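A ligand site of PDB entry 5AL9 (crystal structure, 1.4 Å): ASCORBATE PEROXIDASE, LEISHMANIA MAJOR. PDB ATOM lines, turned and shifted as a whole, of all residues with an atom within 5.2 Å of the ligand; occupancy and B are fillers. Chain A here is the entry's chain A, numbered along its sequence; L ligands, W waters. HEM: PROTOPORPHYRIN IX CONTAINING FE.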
ATOM      1  N   GLU A  24       8.023  -0.036  22.370  1.00  0.00           N
ATOM      2  CA  GLU A  24       7.635  -0.350  20.990  1.00  0.00           C
ATOM      3  C   GLU A  24       7.031   0.846  20.256  1.00  0.00           C
ATOM      4  O   GLU A  24       6.869   0.841  19.028  1.00  0.00           O
ATOM      5  CB  GLU A  24       6.696  -1.571  20.928  1.00  0.00           C
ATOM      6  CG  GLU A  24       5.461  -1.464  21.780  1.00  0.00           C
ATOM      7  CD  GLU A  24       5.718  -1.802  23.245  1.00  0.00           C
ATOM      8  OE1 GLU A  24       6.862  -2.144  23.606  1.00  0.00           O
ATOM      9  OE2 GLU A  24       4.752  -1.723  24.026  1.00  0.00           O
ATOM     10  N   PRO A  27       9.726   2.539  17.313  1.00  0.00           N
ATOM     11  CA  PRO A  27       9.694   2.223  15.886  1.00  0.00           C
ATOM     12  C   PRO A  27       8.390   2.662  15.216  1.00  0.00           C
ATOM     13  O   PRO A  27       8.459   3.069  14.053  1.00  0.00           O
ATOM     14  CB  PRO A  27       9.844   0.696  15.881  1.00  0.00           C
ATOM     15  CG  PRO A  27      10.640   0.409  17.129  1.00  0.00           C
ATOM     16  CD  PRO A  27      10.076   1.370  18.142  1.00  0.00           C
ATOM     17  N   SER A  28       7.261   2.631  15.920  1.00  0.00           N
ATOM     18  CA  SER A  28       6.015   3.054  15.280  1.00  0.00           C
ATOM     19  C   SER A  28       6.040   4.549  14.957  1.00  0.00           C
ATOM     20  O   SER A  28       5.421   4.972  13.985  1.00  0.00           O
ATOM     21  CB  SER A  28       4.781   2.700  16.111  1.00  0.00           C
ATOM     22  OG  SER A  28       4.665   3.525  17.253  1.00  0.00           O
ATOM     23  N   ILE A  30       8.684   6.192  14.001  1.00  0.00           N
ATOM     24  CA  ILE A  30       9.481   6.303  12.782  1.00  0.00           C
ATOM     25  C   ILE A  30       8.617   5.944  11.582  1.00  0.00           C
ATOM     26  O   ILE A  30       8.617   6.628  10.552  1.00  0.00           O
ATOM     27  CB  ILE A  30      10.710   5.411  12.847  1.00  0.00           C
ATOM     28  CG1 ILE A  30      11.624   5.879  13.970  1.00  0.00           C
ATOM     29  CG2 ILE A  30      11.452   5.424  11.524  1.00  0.00           C
ATOM     30  CD1 ILE A  30      12.748   4.932  14.272  1.00  0.00           C
ATOM     31  N   ARG A  31       7.850   4.866  11.720  1.00  0.00           N
ATOM     32  CA  ARG A  31       6.962   4.436  10.638  1.00  0.00           C
ATOM     33  C   ARG A  31       5.938   5.516  10.309  1.00  0.00           C
ATOM     34  O   ARG A  31       5.661   5.765   9.135  1.00  0.00           O
ATOM     35  CB  ARG A  31       6.270   3.110  10.996  1.00  0.00           C
ATOM     36  CG  ARG A  31       5.414   2.565   9.862  1.00  0.00           C
ATOM     37  CD  ARG A  31       4.674   1.303  10.270  1.00  0.00           C
ATOM     38  NE  ARG A  31       3.583   1.049   9.325  1.00  0.00           N
ATOM     39  CZ  ARG A  31       2.357   0.655   9.655  1.00  0.00           C
ATOM     40  NH1 ARG A  31       2.029   0.440  10.925  1.00  0.00           N
ATOM     41  NH2 ARG A  31       1.449   0.499   8.695  1.00  0.00           N
ATOM     42  N   TRP A  34       7.528   8.370   8.367  1.00  0.00           N
ATOM     43  CA  TRP A  34       7.833   7.888   7.027  1.00  0.00           C
ATOM     44  C   TRP A  34       6.574   7.791   6.144  1.00  0.00           C
ATOM     45  O   TRP A  34       6.577   8.261   5.008  1.00  0.00           O
ATOM     46  CB  TRP A  34       8.656   6.601   7.128  1.00  0.00           C
ATOM     47  CG  TRP A  34       8.344   5.532   6.133  1.00  0.00           C
ATOM     48  CD1 TRP A  34       7.836   4.294   6.416  1.00  0.00           C
ATOM     49  CD2 TRP A  34       8.567   5.550   4.714  1.00  0.00           C
ATOM     50  NE1 TRP A  34       7.716   3.561   5.274  1.00  0.00           N
ATOM     51  CE2 TRP A  34       8.150   4.305   4.215  1.00  0.00           C
ATOM     52  CE3 TRP A  34       9.082   6.501   3.830  1.00  0.00           C
ATOM     53  CZ2 TRP A  34       8.222   3.973   2.862  1.00  0.00           C
ATOM     54  CZ3 TRP A  34       9.148   6.171   2.490  1.00  0.00           C
ATOM     55  CH2 TRP A  34       8.724   4.920   2.013  1.00  0.00           C
ATOM     56  N   PRO A 129       4.742   1.769  -0.378  1.00  0.00           N
ATOM     57  CA  PRO A 129       5.303   0.527  -0.920  1.00  0.00           C
ATOM     58  C   PRO A 129       4.626  -0.726  -0.367  1.00  0.00           C
ATOM     59  O   PRO A 129       3.976  -0.706   0.687  1.00  0.00           O
ATOM     60  CB  PRO A 129       6.781   0.588  -0.525  1.00  0.00           C
ATOM     61  CG  PRO A 129       6.801   1.456   0.683  1.00  0.00           C
ATOM     62  CD  PRO A 129       5.727   2.490   0.453  1.00  0.00           C
ATOM     63  N   ASP A 130       4.795  -1.816  -1.096  1.00  0.00           N
ATOM     64  CA  ASP A 130       4.138  -3.077  -0.810  1.00  0.00           C
ATOM     65  C   ASP A 130       5.248  -4.072  -0.487  1.00  0.00           C
ATOM     66  O   ASP A 130       6.110  -4.335  -1.332  1.00  0.00           O
ATOM     67  CB  ASP A 130       3.375  -3.527  -2.061  1.00  0.00           C
ATOM     68  CG  ASP A 130       2.510  -4.758  -1.835  1.00  0.00           C
ATOM     69  OD1 ASP A 130       2.827  -5.574  -0.956  1.00  0.00           O
ATOM     70  OD2 ASP A 130       1.514  -4.898  -2.575  1.00  0.00           O
ATOM     71  N   GLY A 131       5.205  -4.631   0.717  1.00  0.00           N
ATOM     72  CA  GLY A 131       6.237  -5.532   1.196  1.00  0.00           C
ATOM     73  C   GLY A 131       6.321  -6.838   0.443  1.00  0.00           C
ATOM     74  O   GLY A 131       7.333  -7.543   0.525  1.00  0.00           O
ATOM     75  N   VAL A 138      10.055  -1.252  -5.590  1.00  0.00           N
ATOM     76  CA  VAL A 138      10.767  -0.427  -4.620  1.00  0.00           C
ATOM     77  C   VAL A 138      11.427   0.758  -5.314  1.00  0.00           C
ATOM     78  O   VAL A 138      11.301   1.899  -4.872  1.00  0.00           O
ATOM     79  CB  VAL A 138      11.830  -1.255  -3.852  1.00  0.00           C
ATOM     80  CG1 VAL A 138      12.711  -0.350  -3.016  1.00  0.00           C
ATOM     81  CG2 VAL A 138      11.148  -2.296  -2.965  1.00  0.00           C
ATOM     82  N   PHE A 142      10.634   4.768  -4.703  1.00  0.00           N
ATOM     83  CA  PHE A 142      11.647   5.682  -4.208  1.00  0.00           C
ATOM     84  C   PHE A 142      12.077   6.710  -5.243  1.00  0.00           C
ATOM     85  O   PHE A 142      12.383   7.843  -4.877  1.00  0.00           O
ATOM     86  CB  PHE A 142      12.808   4.913  -3.593  1.00  0.00           C
ATOM     87  CG  PHE A 142      12.498   4.429  -2.209  1.00  0.00           C
ATOM     88  CD1 PHE A 142      11.759   3.272  -2.017  1.00  0.00           C
ATOM     89  CD2 PHE A 142      12.916   5.153  -1.107  1.00  0.00           C
ATOM     90  CE1 PHE A 142      11.465   2.836  -0.725  1.00  0.00           C
ATOM     91  CE2 PHE A 142      12.632   4.737   0.176  1.00  0.00           C
ATOM     92  CZ  PHE A 142      11.903   3.562   0.370  1.00  0.00           C
ATOM     93  N   LEU A 155      17.442   4.141   3.874  1.00  0.00           N
ATOM     94  CA  LEU A 155      16.143   4.312   4.524  1.00  0.00           C
ATOM     95  C   LEU A 155      15.503   3.000   4.941  1.00  0.00           C
ATOM     96  O   LEU A 155      14.948   2.893   6.037  1.00  0.00           O
ATOM     97  CB  LEU A 155      15.188   5.112   3.628  1.00  0.00           C
ATOM     98  CG  LEU A 155      15.521   6.595   3.564  1.00  0.00           C
ATOM     99  CD1 LEU A 155      14.729   7.247   2.443  1.00  0.00           C
ATOM    100  CD2 LEU A 155      15.216   7.247   4.894  1.00  0.00           C
ATOM    101  N   ILE A 156      15.602   1.988   4.083  1.00  0.00           N
ATOM    102  CA  ILE A 156      14.971   0.702   4.387  1.00  0.00           C
ATOM    103  C   ILE A 156      15.684   0.026   5.565  1.00  0.00           C
ATOM    104  O   ILE A 156      15.111  -0.799   6.258  1.00  0.00           O
ATOM    105  CB  ILE A 156      14.887  -0.176   3.122  1.00  0.00           C
ATOM    106  CG1 ILE A 156      13.978   0.499   2.094  1.00  0.00           C
ATOM    107  CG2 ILE A 156      14.353  -1.580   3.457  1.00  0.00           C
ATOM    108  CD1 ILE A 156      14.029  -0.132   0.709  1.00  0.00           C
ATOM    109  N   ALA A 158      15.950   1.200   8.281  1.00  0.00           N
ATOM    110  CA  ALA A 158      15.140   1.473   9.473  1.00  0.00           C
ATOM    111  C   ALA A 158      14.460   0.209   9.995  1.00  0.00           C
ATOM    112  O   ALA A 158      14.040   0.184  11.146  1.00  0.00           O
ATOM    113  CB  ALA A 158      14.100   2.528   9.158  1.00  0.00           C
ATOM    114  N   HIS A 159      14.333  -0.827   9.161  1.00  0.00           N
ATOM    115  CA  HIS A 159      13.752  -2.099   9.595  1.00  0.00           C
ATOM    116  C   HIS A 159      14.621  -2.806  10.636  1.00  0.00           C
ATOM    117  O   HIS A 159      14.238  -3.835  11.193  1.00  0.00           O
ATOM    118  CB  HIS A 159      13.418  -2.996   8.398  1.00  0.00           C
ATOM    119  CG  HIS A 159      12.227  -2.527   7.628  1.00  0.00           C
ATOM    120  ND1 HIS A 159      11.846  -3.080   6.421  1.00  0.00           N
ATOM    121  CD2 HIS A 159      11.296  -1.587   7.921  1.00  0.00           C
ATOM    122  CE1 HIS A 159      10.753  -2.462   5.992  1.00  0.00           C
ATOM    123  NE2 HIS A 159      10.398  -1.563   6.883  1.00  0.00           N
ATOM    124  N   CYS A 161      14.769  -1.553  13.320  1.00  0.00           N
ATOM    125  CA  CYS A 161      13.881  -1.193  14.432  1.00  0.00           C
ATOM    126  C   CYS A 161      12.507  -1.790  14.190  1.00  0.00           C
ATOM    127  O   CYS A 161      12.012  -1.775  13.071  1.00  0.00           O
ATOM    128  CB  CYS A 161      13.755   0.347  14.531  1.00  0.00           C
ATOM    129  SG  CYS A 161      15.229   1.137  15.198  1.00  0.00           S
ATOM    130  N   GLY A 162      11.882  -2.275  15.260  1.00  0.00           N
ATOM    131  CA  GLY A 162      10.489  -2.656  15.195  1.00  0.00           C
ATOM    132  C   GLY A 162      10.163  -4.022  14.663  1.00  0.00           C
ATOM    133  O   GLY A 162      11.011  -4.906  14.549  1.00  0.00           O
ATOM    134  N   GLU A 163       8.906  -4.186  14.296  1.00  0.00           N
ATOM    135  CA  GLU A 163       8.411  -5.498  13.953  1.00  0.00           C
ATOM    136  C   GLU A 163       7.134  -5.375  13.158  1.00  0.00           C
ATOM    137  O   GLU A 163       6.504  -4.319  13.105  1.00  0.00           O
ATOM    138  CB  GLU A 163       8.150  -6.300  15.222  1.00  0.00           C
ATOM    139  CG  GLU A 163       7.104  -5.687  16.130  1.00  0.00           C
ATOM    140  CD  GLU A 163       7.110  -6.295  17.510  1.00  0.00           C
ATOM    141  OE1 GLU A 163       7.033  -7.534  17.612  1.00  0.00           O
ATOM    142  OE2 GLU A 163       7.208  -5.530  18.500  1.00  0.00           O
ATOM    143  N   CYS A 164       6.787  -6.483  12.522  1.00  0.00           N
ATOM    144  CA  CYS A 164       5.537  -6.601  11.799  1.00  0.00           C
ATOM    145  C   CYS A 164       4.465  -7.172  12.699  1.00  0.00           C
ATOM    146  O   CYS A 164       4.717  -8.049  13.540  1.00  0.00           O
ATOM    147  CB  CYS A 164       5.713  -7.507  10.592  1.00  0.00           C
ATOM    148  SG  CYS A 164       6.739  -6.812   9.300  1.00  0.00           S
ATOM    149  N   HIS A 165       3.243  -6.701  12.502  1.00  0.00           N
ATOM    150  CA  HIS A 165       2.099  -7.161  13.256  1.00  0.00           C
ATOM    151  C   HIS A 165       1.077  -7.758  12.314  1.00  0.00           C
ATOM    152  O   HIS A 165       0.712  -7.146  11.306  1.00  0.00           O
ATOM    153  CB  HIS A 165       1.464  -5.986  13.995  1.00  0.00           C
ATOM    154  CG  HIS A 165       2.444  -5.212  14.819  1.00  0.00           C
ATOM    155  ND1 HIS A 165       3.215  -4.206  14.297  1.00  0.00           N
ATOM    156  CD2 HIS A 165       2.768  -5.303  16.126  1.00  0.00           C
ATOM    157  CE1 HIS A 165       3.978  -3.695  15.248  1.00  0.00           C
ATOM    158  NE2 HIS A 165       3.731  -4.347  16.368  1.00  0.00           N
ATOM    159  N   ILE A 166       0.614  -8.957  12.632  1.00  0.00           N
ATOM    160  CA  ILE A 166      -0.353  -9.643  11.777  1.00  0.00           C
ATOM    161  C   ILE A 166      -1.564  -8.758  11.515  1.00  0.00           C
ATOM    162  O   ILE A 166      -2.064  -8.690  10.388  1.00  0.00           O
ATOM    163  CB  ILE A 166      -0.803 -10.966  12.423  1.00  0.00           C
ATOM    164  CG1 ILE A 166       0.369 -11.949  12.422  1.00  0.00           C
ATOM    165  CG2 ILE A 166      -2.008 -11.556  11.692  1.00  0.00           C
ATOM    166  CD1 ILE A 166       0.196 -13.136  13.332  1.00  0.00           C
ATOM    167  N   PHE A 168      -1.764  -5.636  11.289  1.00  0.00           N
ATOM    168  CA  PHE A 168      -1.541  -4.425  10.498  1.00  0.00           C
ATOM    169  C   PHE A 168      -1.127  -4.707   9.078  1.00  0.00           C
ATOM    170  O   PHE A 168      -1.633  -4.076   8.145  1.00  0.00           O
ATOM    171  CB  PHE A 168      -0.513  -3.512  11.175  1.00  0.00           C
ATOM    172  CG  PHE A 168      -0.890  -3.088  12.561  1.00  0.00           C
ATOM    173  CD1 PHE A 168      -2.218  -3.044  12.960  1.00  0.00           C
ATOM    174  CD2 PHE A 168       0.088  -2.731  13.478  1.00  0.00           C
ATOM    175  CE1 PHE A 168      -2.573  -2.653  14.244  1.00  0.00           C
ATOM    176  CE2 PHE A 168      -0.255  -2.353  14.771  1.00  0.00           C
ATOM    177  CZ  PHE A 168      -1.587  -2.319  15.139  1.00  0.00           C
ATOM    178  N   SER A 169      -0.207  -5.643   8.898  1.00  0.00           N
ATOM    179  CA  SER A 169       0.344  -5.925   7.571  1.00  0.00           C
ATOM    180  C   SER A 169       0.186  -7.381   7.167  1.00  0.00           C
ATOM    181  O   SER A 169       0.457  -7.736   6.011  1.00  0.00           O
ATOM    182  CB  SER A 169       1.828  -5.590   7.529  1.00  0.00           C
ATOM    183  OG  SER A 169       2.546  -6.428   8.425  1.00  0.00           O
ATOM    184  N   GLY A 170      -0.219  -8.228   8.106  1.00  0.00           N
ATOM    185  CA  GLY A 170      -0.295  -9.653   7.850  1.00  0.00           C
ATOM    186  C   GLY A 170       1.034 -10.365   8.026  1.00  0.00           C
ATOM    187  O   GLY A 170       1.072 -11.582   7.992  1.00  0.00           O
ATOM    188  N   TYR A 171       2.113  -9.613   8.194  1.00  0.00           N
ATOM    189  CA  TYR A 171       3.422 -10.222   8.432  1.00  0.00           C
ATOM    190  C   TYR A 171       3.622 -10.326   9.925  1.00  0.00           C
ATOM    191  O   TYR A 171       2.909  -9.683  10.705  1.00  0.00           O
ATOM    192  CB  TYR A 171       4.520  -9.367   7.830  1.00  0.00           C
ATOM    193  CG  TYR A 171       4.481  -9.316   6.319  1.00  0.00           C
ATOM    194  CD1 TYR A 171       4.810 -10.420   5.561  1.00  0.00           C
ATOM    195  CD2 TYR A 171       4.133  -8.136   5.662  1.00  0.00           C
ATOM    196  CE1 TYR A 171       4.789 -10.374   4.177  1.00  0.00           C
ATOM    197  CE2 TYR A 171       4.109  -8.070   4.288  1.00  0.00           C
ATOM    198  CZ  TYR A 171       4.438  -9.187   3.558  1.00  0.00           C
ATOM    199  OH  TYR A 171       4.411  -9.138   2.186  1.00  0.00           O
ATOM    200  N   TRP A 175      12.479  -7.902  12.429  1.00  0.00           N
ATOM    201  CA  TRP A 175      13.500  -8.217  11.436  1.00  0.00           C
ATOM    202  C   TRP A 175      14.728  -8.727  12.138  1.00  0.00           C
ATOM    203  O   TRP A 175      15.231  -9.787  11.803  1.00  0.00           O
ATOM    204  CB  TRP A 175      13.842  -6.999  10.594  1.00  0.00           C
ATOM    205  CG  TRP A 175      12.810  -6.652   9.576  1.00  0.00           C
ATOM    206  CD1 TRP A 175      12.775  -7.041   8.276  1.00  0.00           C
ATOM    207  CD2 TRP A 175      11.655  -5.837   9.792  1.00  0.00           C
ATOM    208  NE1 TRP A 175      11.664  -6.513   7.654  1.00  0.00           N
ATOM    209  CE2 TRP A 175      10.967  -5.761   8.565  1.00  0.00           C
ATOM    210  CE3 TRP A 175      11.144  -5.143  10.894  1.00  0.00           C
ATOM    211  CZ2 TRP A 175       9.779  -5.044   8.417  1.00  0.00           C
ATOM    212  CZ3 TRP A 175       9.979  -4.418  10.747  1.00  0.00           C
ATOM    213  CH2 TRP A 175       9.307  -4.374   9.519  1.00  0.00           C
ATOM    214  N   LEU A 217      11.119  -9.500   4.544  1.00  0.00           N
ATOM    215  CA  LEU A 217      10.059  -9.435   3.551  1.00  0.00           C
ATOM    216  C   LEU A 217      10.663  -9.594   2.162  1.00  0.00           C
ATOM    217  O   LEU A 217      11.864  -9.408   1.983  1.00  0.00           O
ATOM    218  CB  LEU A 217       9.386  -8.074   3.609  1.00  0.00           C
ATOM    219  CG  LEU A 217       8.846  -7.527   4.932  1.00  0.00           C
ATOM    220  CD1 LEU A 217       8.584  -6.034   4.800  1.00  0.00           C
ATOM    221  CD2 LEU A 217       7.586  -8.256   5.313  1.00  0.00           C
ATOM    222  N   SER A 219      10.366  -7.431  -0.084  1.00  0.00           N
ATOM    223  CA  SER A 219      10.911  -6.110  -0.371  1.00  0.00           C
ATOM    224  C   SER A 219      12.257  -5.869   0.294  1.00  0.00           C
ATOM    225  O   SER A 219      13.046  -5.038  -0.161  1.00  0.00           O
ATOM    226  CB  SER A 219       9.907  -5.017   0.019  1.00  0.00           C
ATOM    227  OG  SER A 219       9.523  -5.138   1.368  1.00  0.00           O
ATOM    228  N   PHE A 247      21.733   7.435   6.811  1.00  0.00           N
ATOM    229  CA  PHE A 247      20.349   7.389   7.255  1.00  0.00           C
ATOM    230  C   PHE A 247      19.894   8.754   7.749  1.00  0.00           C
ATOM    231  O   PHE A 247      18.793   9.192   7.440  1.00  0.00           O
ATOM    232  CB  PHE A 247      20.144   6.362   8.373  1.00  0.00           C
ATOM    233  CG  PHE A 247      18.715   6.247   8.782  1.00  0.00           C
ATOM    234  CD1 PHE A 247      17.866   5.418   8.077  1.00  0.00           C
ATOM    235  CD2 PHE A 247      18.209   6.991   9.835  1.00  0.00           C
ATOM    236  CE1 PHE A 247      16.524   5.331   8.423  1.00  0.00           C
ATOM    237  CE2 PHE A 247      16.874   6.898  10.185  1.00  0.00           C
ATOM    238  CZ  PHE A 247      16.031   6.063   9.484  1.00  0.00           C
ATOM    239  N   PHE A 251      16.815  10.512   5.963  1.00  0.00           N
ATOM    240  CA  PHE A 251      15.599  10.680   6.738  1.00  0.00           C
ATOM    241  C   PHE A 251      15.250  12.149   6.906  1.00  0.00           C
ATOM    242  O   PHE A 251      14.071  12.524   6.918  1.00  0.00           O
ATOM    243  CB  PHE A 251      15.691   9.963   8.087  1.00  0.00           C
ATOM    244  CG  PHE A 251      14.366   9.743   8.742  1.00  0.00           C
ATOM    245  CD1 PHE A 251      13.539   8.713   8.310  1.00  0.00           C
ATOM    246  CD2 PHE A 251      13.923  10.567   9.771  1.00  0.00           C
ATOM    247  CE1 PHE A 251      12.305   8.508   8.899  1.00  0.00           C
ATOM    248  CE2 PHE A 251      12.687  10.352  10.369  1.00  0.00           C
ATOM    249  CZ  PHE A 251      11.874   9.320   9.936  1.00  0.00           C
ATOM    250  N   LEU A 254      13.710  13.050   3.641  1.00  0.00           N
ATOM    251  CA  LEU A 254      12.374  12.470   3.571  1.00  0.00           C
ATOM    252  C   LEU A 254      11.368  13.344   4.314  1.00  0.00           C
ATOM    253  O   LEU A 254      10.294  13.665   3.799  1.00  0.00           O
ATOM    254  CB  LEU A 254      12.418  11.084   4.222  1.00  0.00           C
ATOM    255  CG  LEU A 254      11.092  10.345   4.345  1.00  0.00           C
ATOM    256  CD1 LEU A 254      10.594   9.898   2.982  1.00  0.00           C
ATOM    257  CD2 LEU A 254      11.226   9.158   5.305  1.00  0.00           C
HETATM  258  CHA HEM L   1       7.171  -1.600   9.479  1.00  0.00           C
HETATM  259  CHB HEM L   1       7.024  -2.314   4.714  1.00  0.00           C
HETATM  260  CHC HEM L   1      10.227   1.216   4.052  1.00  0.00           C
HETATM  261  CHD HEM L   1      10.210   2.126   8.767  1.00  0.00           C
HETATM  262  C1A HEM L   1       6.830  -2.081   8.248  1.00  0.00           C
HETATM  263  C2A HEM L   1       5.851  -3.115   7.987  1.00  0.00           C
HETATM  264  C3A HEM L   1       5.809  -3.334   6.667  1.00  0.00           C
HETATM  265  C4A HEM L   1       6.763  -2.427   6.053  1.00  0.00           C
HETATM  266  CMA HEM L   1       4.908  -4.349   5.929  1.00  0.00           C
HETATM  267  CAA HEM L   1       5.037  -3.826   9.084  1.00  0.00           C
HETATM  268  CBA HEM L   1       3.932  -2.931   9.636  1.00  0.00           C
HETATM  269  CGA HEM L   1       3.255  -3.653  10.764  1.00  0.00           C
HETATM  270  O1A HEM L   1       2.797  -4.819  10.553  1.00  0.00           O
HETATM  271  O2A HEM L   1       3.159  -3.067  11.878  1.00  0.00           O
HETATM  272  C1B HEM L   1       7.929  -1.487   4.105  1.00  0.00           C
HETATM  273  C2B HEM L   1       8.366  -1.503   2.733  1.00  0.00           C
HETATM  274  C3B HEM L   1       9.252  -0.505   2.557  1.00  0.00           C
HETATM  275  C4B HEM L   1       9.410   0.149   3.823  1.00  0.00           C
HETATM  276  CMB HEM L   1       7.848  -2.497   1.692  1.00  0.00           C
HETATM  277  CAB HEM L   1      10.050  -0.087   1.295  1.00  0.00           C
HETATM  278  CBB HEM L   1      10.335  -0.918   0.285  1.00  0.00           C
HETATM  279  C1C HEM L   1      10.425   1.834   5.256  1.00  0.00           C
HETATM  280  C2C HEM L   1      11.137   3.088   5.472  1.00  0.00           C
HETATM  281  C3C HEM L   1      11.098   3.342   6.780  1.00  0.00           C
HETATM  282  C4C HEM L   1      10.407   2.249   7.422  1.00  0.00           C
HETATM  283  CMC HEM L   1      11.737   3.943   4.348  1.00  0.00           C
HETATM  284  CAC HEM L   1      11.684   4.509   7.579  1.00  0.00           C
HETATM  285  CBC HEM L   1      12.786   5.159   7.203  1.00  0.00           C
HETATM  286  C1D HEM L   1       9.521   1.126   9.404  1.00  0.00           C
HETATM  287  C2D HEM L   1       9.540   0.853  10.810  1.00  0.00           C
HETATM  288  C3D HEM L   1       8.602  -0.306  11.042  1.00  0.00           C
HETATM  289  C4D HEM L   1       8.090  -0.617   9.734  1.00  0.00           C
HETATM  290  CMD HEM L   1      10.364   1.565  11.889  1.00  0.00           C
HETATM  291  CAD HEM L   1       8.302  -0.963  12.393  1.00  0.00           C
HETATM  292  CBD HEM L   1       6.984  -0.399  12.923  1.00  0.00           C
HETATM  293  CGD HEM L   1       6.623  -0.920  14.285  1.00  0.00           C
HETATM  294  O1D HEM L   1       7.454  -1.616  14.942  1.00  0.00           O
HETATM  295  O2D HEM L   1       5.495  -0.636  14.753  1.00  0.00           O
HETATM  296  NA  HEM L   1       7.372  -1.665   7.040  1.00  0.00           N
HETATM  297  NB  HEM L   1       8.591  -0.467   4.744  1.00  0.00           N
HETATM  298  NC  HEM L   1       9.977   1.344   6.470  1.00  0.00           N
HETATM  299  ND  HEM L   1       8.662   0.234   8.805  1.00  0.00           N
HETATM  300 FE   HEM L   1       8.766  -0.248   6.781  1.00  0.00          FE
HETATM  301  O   HOH W   1       6.976   0.979   6.536  1.00  0.00           O
HETATM  302  O   HOH W   2       3.455  -0.556  13.037  1.00  0.00           O
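Water W2 bridges an oxygen (O2D) of the ligand (2.7 Å) and the guanidinium group (NH1) of Arg 31 (2.7 Å).
O2A of the ligand is in hydrogen-bond range of ND1 of His 165 (2.7 Å).
The side-chain hydroxyl (OG) of Ser 169 sits at hydrogen-bond distance from an oxygen (O1A) of the ligand (2.7 Å).
NE2 of His 159 is bound to FE of the ligand, 2.1 Å away.
N of Glu 163 is in hydrogen-bond range of O1D of the ligand, at 3.0 Å.
An oxygen (O1A) of the ligand is in hydrogen-bond range of the backbone NH (N) of His 165.
The guanidinium group of Arg 31 lies within salt-bridge range of an oxygen (O2A) of the ligand (3.8 Å).
The indole nitrogen (NE1) of Trp 34 lies close to a nitrogen (NC) of the ligand, 3.4 Å away.
Merely in contact with the ligand: Ser 219, Gly 162, Pro 27, Leu 155, Cys 164, Gly 131, Phe 168, Ala 158, Trp 175, Val 138, Pro 129, Ser 28, Asp 130, Phe 251, Ile 156, Phe 142, Cys 161, Tyr 171, Phe 247 and Ile 30.
Of the 31 residues printed, 26 come within 4 Å of the ligand.
The backbone NH of Ser 219 is in hydrogen-bond range of the backbone carbonyl oxygen of Gly 131 (3.1 Å).
The backbone NH of Tyr 171 sits close to the side-chain hydroxyl of Ser 169 (3.2 Å).
The backbone carbonyl oxygen (O) of Tyr 171 is in hydrogen-bond range of the backbone NH (N) of Ile 166.
O of His 165 lies within hydrogen-bond range of OG of Ser 169 (3.5 Å).
The backbone NH (N) of His 165 sits close to the backbone carbonyl oxygen (O) of Tyr 171 (3.5 Å).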
